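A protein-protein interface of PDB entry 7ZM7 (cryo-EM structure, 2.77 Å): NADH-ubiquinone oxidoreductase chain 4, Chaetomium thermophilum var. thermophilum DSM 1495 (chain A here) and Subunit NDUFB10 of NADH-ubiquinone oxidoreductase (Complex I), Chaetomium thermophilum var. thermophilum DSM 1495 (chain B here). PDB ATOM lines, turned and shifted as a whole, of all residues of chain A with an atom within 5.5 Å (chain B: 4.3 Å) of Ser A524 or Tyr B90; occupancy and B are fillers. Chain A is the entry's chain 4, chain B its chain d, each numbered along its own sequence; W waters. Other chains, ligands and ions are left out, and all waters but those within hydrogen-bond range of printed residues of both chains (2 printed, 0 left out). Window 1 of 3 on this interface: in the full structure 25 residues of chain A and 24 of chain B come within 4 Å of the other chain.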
ATOM      1  N   PRO A 305      23.192   6.759  16.115  1.00  0.00           N
ATOM      2  CA  PRO A 305      22.267   5.847  15.434  1.00  0.00           C
ATOM      3  C   PRO A 305      20.937   6.446  14.988  1.00  0.00           C
ATOM      4  O   PRO A 305      20.357   5.949  14.024  1.00  0.00           O
ATOM      5  CB  PRO A 305      22.060   4.748  16.478  1.00  0.00           C
ATOM      6  CG  PRO A 305      22.178   5.425  17.732  1.00  0.00           C
ATOM      7  CD  PRO A 305      23.143   6.559  17.572  1.00  0.00           C
ATOM      8  N   TYR A 520      32.694  -5.113  17.443  1.00  0.00           N
ATOM      9  CA  TYR A 520      31.386  -5.498  16.856  1.00  0.00           C
ATOM     10  C   TYR A 520      30.290  -4.469  17.160  1.00  0.00           C
ATOM     11  O   TYR A 520      29.536  -4.115  16.246  1.00  0.00           O
ATOM     12  CB  TYR A 520      31.002  -6.904  17.316  1.00  0.00           C
ATOM     13  CG  TYR A 520      29.768  -7.407  16.628  1.00  0.00           C
ATOM     14  CD1 TYR A 520      29.847  -7.935  15.352  1.00  0.00           C
ATOM     15  CD2 TYR A 520      28.528  -7.309  17.231  1.00  0.00           C
ATOM     16  CE1 TYR A 520      28.719  -8.385  14.696  1.00  0.00           C
ATOM     17  CE2 TYR A 520      27.390  -7.752  16.587  1.00  0.00           C
ATOM     18  CZ  TYR A 520      27.491  -8.278  15.315  1.00  0.00           C
ATOM     19  OH  TYR A 520      26.373  -8.678  14.666  1.00  0.00           O
ATOM     20  N   ASN A 521      30.187  -4.028  18.410  1.00  0.00           N
ATOM     21  CA  ASN A 521      29.128  -3.074  18.841  1.00  0.00           C
ATOM     22  C   ASN A 521      29.344  -1.682  18.244  1.00  0.00           C
ATOM     23  O   ASN A 521      28.350  -1.029  17.899  1.00  0.00           O
ATOM     24  CB  ASN A 521      28.945  -3.118  20.360  1.00  0.00           C
ATOM     25  CG  ASN A 521      28.334  -4.429  20.806  1.00  0.00           C
ATOM     26  OD1 ASN A 521      28.870  -5.102  21.681  1.00  0.00           O
ATOM     27  ND2 ASN A 521      27.223  -4.815  20.201  1.00  0.00           N
ATOM     28  N   ILE A 522      30.594  -1.235  18.164  1.00  0.00           N
ATOM     29  CA  ILE A 522      30.903   0.086  17.548  1.00  0.00           C
ATOM     30  C   ILE A 522      30.504   0.001  16.074  1.00  0.00           C
ATOM     31  O   ILE A 522      30.145   1.035  15.497  1.00  0.00           O
ATOM     32  CB  ILE A 522      32.381   0.486  17.761  1.00  0.00           C
ATOM     33  CG1 ILE A 522      32.530   1.960  18.144  1.00  0.00           C
ATOM     34  CG2 ILE A 522      33.254   0.115  16.572  1.00  0.00           C
ATOM     35  CD1 ILE A 522      32.157   2.259  19.570  1.00  0.00           C
ATOM     36  N   SER A 523      30.605  -1.185  15.483  1.00  0.00           N
ATOM     37  CA  SER A 523      30.306  -1.354  14.042  1.00  0.00           C
ATOM     38  C   SER A 523      28.831  -1.153  13.718  1.00  0.00           C
ATOM     39  O   SER A 523      28.471  -1.304  12.548  1.00  0.00           O
ATOM     40  CB  SER A 523      30.737  -2.723  13.578  1.00  0.00           C
ATOM     41  OG  SER A 523      32.148  -2.843  13.607  1.00  0.00           O
ATOM     42  N   SER A 524      28.023  -0.756  14.705  1.00  0.00           N
ATOM     43  CA  SER A 524      26.643  -0.421  14.402  1.00  0.00           C
ATOM     44  C   SER A 524      26.307   1.048  14.621  1.00  0.00           C
ATOM     45  O   SER A 524      25.127   1.397  14.583  1.00  0.00           O
ATOM     46  CB  SER A 524      25.708  -1.309  15.217  1.00  0.00           C
ATOM     47  OG  SER A 524      25.956  -1.198  16.598  1.00  0.00           O
ATOM     48  N   VAL A 525      27.285   1.920  14.839  1.00  0.00           N
ATOM     49  CA  VAL A 525      27.025   3.355  14.812  1.00  0.00           C
ATOM     50  C   VAL A 525      27.648   4.035  13.617  1.00  0.00           C
ATOM     51  O   VAL A 525      27.560   5.261  13.521  1.00  0.00           O
ATOM     52  CB  VAL A 525      27.468   4.068  16.109  1.00  0.00           C
ATOM     53  CG1 VAL A 525      26.594   3.673  17.266  1.00  0.00           C
ATOM     54  CG2 VAL A 525      28.926   3.789  16.423  1.00  0.00           C
ATOM     55  N   VAL A 526      28.260   3.301  12.700  1.00  0.00           N
ATOM     56  CA  VAL A 526      28.812   3.930  11.500  1.00  0.00           C
ATOM     57  C   VAL A 526      27.721   4.089  10.452  1.00  0.00           C
ATOM     58  O   VAL A 526      26.899   3.197  10.243  1.00  0.00           O
ATOM     59  CB  VAL A 526      30.006   3.136  10.942  1.00  0.00           C
ATOM     60  CG1 VAL A 526      30.607   3.888   9.796  1.00  0.00           C
ATOM     61  CG2 VAL A 526      31.055   2.905  11.997  1.00  0.00           C
ATOM     62  N   PHE B  20      18.018  -6.256   3.616  1.00  0.00           N
ATOM     63  CA  PHE B  20      16.798  -5.854   4.277  1.00  0.00           C
ATOM     64  C   PHE B  20      15.596  -5.992   3.366  1.00  0.00           C
ATOM     65  O   PHE B  20      14.470  -5.773   3.821  1.00  0.00           O
ATOM     66  CB  PHE B  20      16.911  -4.413   4.780  1.00  0.00           C
ATOM     67  CG  PHE B  20      17.804  -4.272   5.958  1.00  0.00           C
ATOM     68  CD1 PHE B  20      17.394  -4.699   7.203  1.00  0.00           C
ATOM     69  CD2 PHE B  20      19.062  -3.754   5.827  1.00  0.00           C
ATOM     70  CE1 PHE B  20      18.218  -4.586   8.282  1.00  0.00           C
ATOM     71  CE2 PHE B  20      19.882  -3.654   6.912  1.00  0.00           C
ATOM     72  CZ  PHE B  20      19.454  -4.068   8.132  1.00  0.00           C
ATOM     73  N   GLN B  35      20.720  -7.274  10.498  1.00  0.00           N
ATOM     74  CA  GLN B  35      21.804  -6.372  10.873  1.00  0.00           C
ATOM     75  C   GLN B  35      23.090  -7.144  11.100  1.00  0.00           C
ATOM     76  O   GLN B  35      24.142  -6.772  10.578  1.00  0.00           O
ATOM     77  CB  GLN B  35      21.444  -5.592  12.134  1.00  0.00           C
ATOM     78  CG  GLN B  35      20.303  -4.628  12.012  1.00  0.00           C
ATOM     79  CD  GLN B  35      19.745  -4.262  13.357  1.00  0.00           C
ATOM     80  OE1 GLN B  35      20.057  -4.896  14.346  1.00  0.00           O
ATOM     81  NE2 GLN B  35      18.928  -3.235  13.404  1.00  0.00           N
ATOM     82  N   ILE B  39      26.908  -6.977   9.077  1.00  0.00           N
ATOM     83  CA  ILE B  39      28.121  -6.647   9.821  1.00  0.00           C
ATOM     84  C   ILE B  39      29.199  -7.693   9.584  1.00  0.00           C
ATOM     85  O   ILE B  39      30.379  -7.362   9.444  1.00  0.00           O
ATOM     86  CB  ILE B  39      27.804  -6.486  11.319  1.00  0.00           C
ATOM     87  CG1 ILE B  39      26.921  -5.274  11.538  1.00  0.00           C
ATOM     88  CG2 ILE B  39      29.057  -6.332  12.126  1.00  0.00           C
ATOM     89  CD1 ILE B  39      27.566  -3.977  11.198  1.00  0.00           C
ATOM     90  N   GLY B  89      28.985  -0.350   8.491  1.00  0.00           N
ATOM     91  CA  GLY B  89      27.771  -0.562   9.293  1.00  0.00           C
ATOM     92  C   GLY B  89      26.564  -0.947   8.461  1.00  0.00           C
ATOM     93  O   GLY B  89      26.740  -1.249   7.274  1.00  0.00           O
ATOM     94  N   TYR B  90      25.377  -0.949   9.071  1.00  0.00           N
ATOM     95  CA  TYR B  90      24.137  -1.290   8.395  1.00  0.00           C
ATOM     96  C   TYR B  90      23.156  -0.133   8.380  1.00  0.00           C
ATOM     97  O   TYR B  90      22.129  -0.215   7.709  1.00  0.00           O
ATOM     98  CB  TYR B  90      23.484  -2.497   9.077  1.00  0.00           C
ATOM     99  CG  TYR B  90      23.130  -2.280  10.530  1.00  0.00           C
ATOM    100  CD1 TYR B  90      22.022  -1.533  10.894  1.00  0.00           C
ATOM    101  CD2 TYR B  90      23.893  -2.836  11.535  1.00  0.00           C
ATOM    102  CE1 TYR B  90      21.707  -1.336  12.204  1.00  0.00           C
ATOM    103  CE2 TYR B  90      23.574  -2.645  12.849  1.00  0.00           C
ATOM    104  CZ  TYR B  90      22.479  -1.901  13.175  1.00  0.00           C
ATOM    105  OH  TYR B  90      22.152  -1.703  14.489  1.00  0.00           O
ATOM    106  N   LEU B  91      23.453   0.936   9.105  1.00  0.00           N
ATOM    107  CA  LEU B  91      22.455   1.945   9.406  1.00  0.00           C
ATOM    108  C   LEU B  91      21.967   2.619   8.146  1.00  0.00           C
ATOM    109  O   LEU B  91      20.784   2.944   8.021  1.00  0.00           O
ATOM    110  CB  LEU B  91      23.051   2.970  10.360  1.00  0.00           C
ATOM    111  CG  LEU B  91      22.112   3.958  11.011  1.00  0.00           C
ATOM    112  CD1 LEU B  91      21.158   3.195  11.888  1.00  0.00           C
ATOM    113  CD2 LEU B  91      22.931   4.933  11.801  1.00  0.00           C
ATOM    114  N   PHE B  92      22.870   2.849   7.204  1.00  0.00           N
ATOM    115  CA  PHE B  92      22.466   3.388   5.922  1.00  0.00           C
ATOM    116  C   PHE B  92      21.583   2.410   5.158  1.00  0.00           C
ATOM    117  O   PHE B  92      20.552   2.803   4.610  1.00  0.00           O
ATOM    118  CB  PHE B  92      23.699   3.756   5.109  1.00  0.00           C
ATOM    119  CG  PHE B  92      23.390   4.634   3.969  1.00  0.00           C
ATOM    120  CD1 PHE B  92      22.994   4.094   2.777  1.00  0.00           C
ATOM    121  CD2 PHE B  92      23.410   5.994   4.109  1.00  0.00           C
ATOM    122  CE1 PHE B  92      22.671   4.881   1.749  1.00  0.00           C
ATOM    123  CE2 PHE B  92      23.078   6.795   3.073  1.00  0.00           C
ATOM    124  CZ  PHE B  92      22.711   6.237   1.889  1.00  0.00           C
ATOM    125  N   GLU B  93      21.970   1.137   5.115  1.00  0.00           N
ATOM    126  CA  GLU B  93      21.194   0.132   4.336  1.00  0.00           C
ATOM    127  C   GLU B  93      19.847  -0.145   5.012  1.00  0.00           C
ATOM    128  O   GLU B  93      18.907  -0.496   4.287  1.00  0.00           O
ATOM    129  CB  GLU B  93      21.987  -1.160   4.152  1.00  0.00           C
ATOM    130  CG  GLU B  93      22.833  -1.196   2.896  1.00  0.00           C
ATOM    131  CD  GLU B  93      23.197  -2.608   2.470  1.00  0.00           C
ATOM    132  OE1 GLU B  93      22.274  -3.378   2.137  1.00  0.00           O
ATOM    133  OE2 GLU B  93      24.398  -2.940   2.489  1.00  0.00           O
ATOM    134  N   GLN B  94      19.767  -0.015   6.341  1.00  0.00           N
ATOM    135  CA  GLN B  94      18.509  -0.258   7.038  1.00  0.00           C
ATOM    136  C   GLN B  94      17.484   0.814   6.722  1.00  0.00           C
ATOM    137  O   GLN B  94      16.290   0.530   6.651  1.00  0.00           O
ATOM    138  CB  GLN B  94      18.741  -0.334   8.542  1.00  0.00           C
ATOM    139  CG  GLN B  94      17.570  -0.895   9.302  1.00  0.00           C
ATOM    140  CD  GLN B  94      17.857  -1.081  10.755  1.00  0.00           C
ATOM    141  OE1 GLN B  94      18.441  -2.075  11.153  1.00  0.00           O
ATOM    142  NE2 GLN B  94      17.437  -0.134  11.567  1.00  0.00           N
HETATM  143  O   HOH W   1      26.110   2.700   7.739  1.00  0.00           O
HETATM  144  O   HOH W   2      25.157   0.841  11.699  1.00  0.00           O
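The backbone carbonyl oxygen (O) of Asn A521 is in hydrogen-bond range of the side-chain hydroxyl (OG) of Ser A524, 2.7 Å away.
Leu B91 touches Pro A305. Ile B39 touches Tyr A520. Ser A523 touches Ile B39 (O to CD1, 3.1 Å). Ser A523 touches Gly B89. Ser A524 touches Tyr B90 (CB to CE2, 3.5 Å). O of Val A526 touches CA of Gly B89, at 3.97 Å. Val A526 touches Leu B91 (O to CB, 3.9 Å).
Of the printed residues of chain B, Pro A305 touches Leu B91. Of the printed residues of chain B, Tyr A520 touches Ile B39 (3.3 Å). Ile A522 touches none of the printed residues of chain B. Printed residues of chain B within 4 Å of Ser A523: Ile B39 (3.1 Å) and Gly B89 (3.4 Å). Of the printed residues of chain B, Ser A524 touches Tyr B90 (3.5 Å). Of chain A, only Ser A524 comes within 4 Å of Tyr B90. Phe B92 touches none of the printed residues of chain A. The nearest printed residue of chain B that does not touch Ser A524 is Ile B39 (4.8 Å). The nearest printed residue of chain B that does not touch Ser A523 is Tyr B90 (4.7 Å).
Of the 8 printed residues of chain A, 5 touch a printed residue of chain B. Hydrophobic or aromatic side chains of chain A that line the printed part of chain B: Tyr A520. Of the 9 printed residues of chain B, 4 touch a printed residue of chain A. Hydrophobic or aromatic side chains of chain B that line the printed part of chain A: Ile B39, Tyr B90 and Leu B91. Among the printed residues, 7 pairs touch across the chains.
Water W1 lies within hydrogen-bond range of O of Val A526, N of Phe B92 and N of Leu B91. Water W2 lies within hydrogen-bond range of the backbone carbonyl oxygen (O) of Ser A524 (2.9 Å), the backbone NH (N) of Leu B91 (3.1 Å), the backbone NH (N) of Tyr B90 (3.2 Å) and the backbone carbonyl oxygen (O) of Val A526 (3.3 Å).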
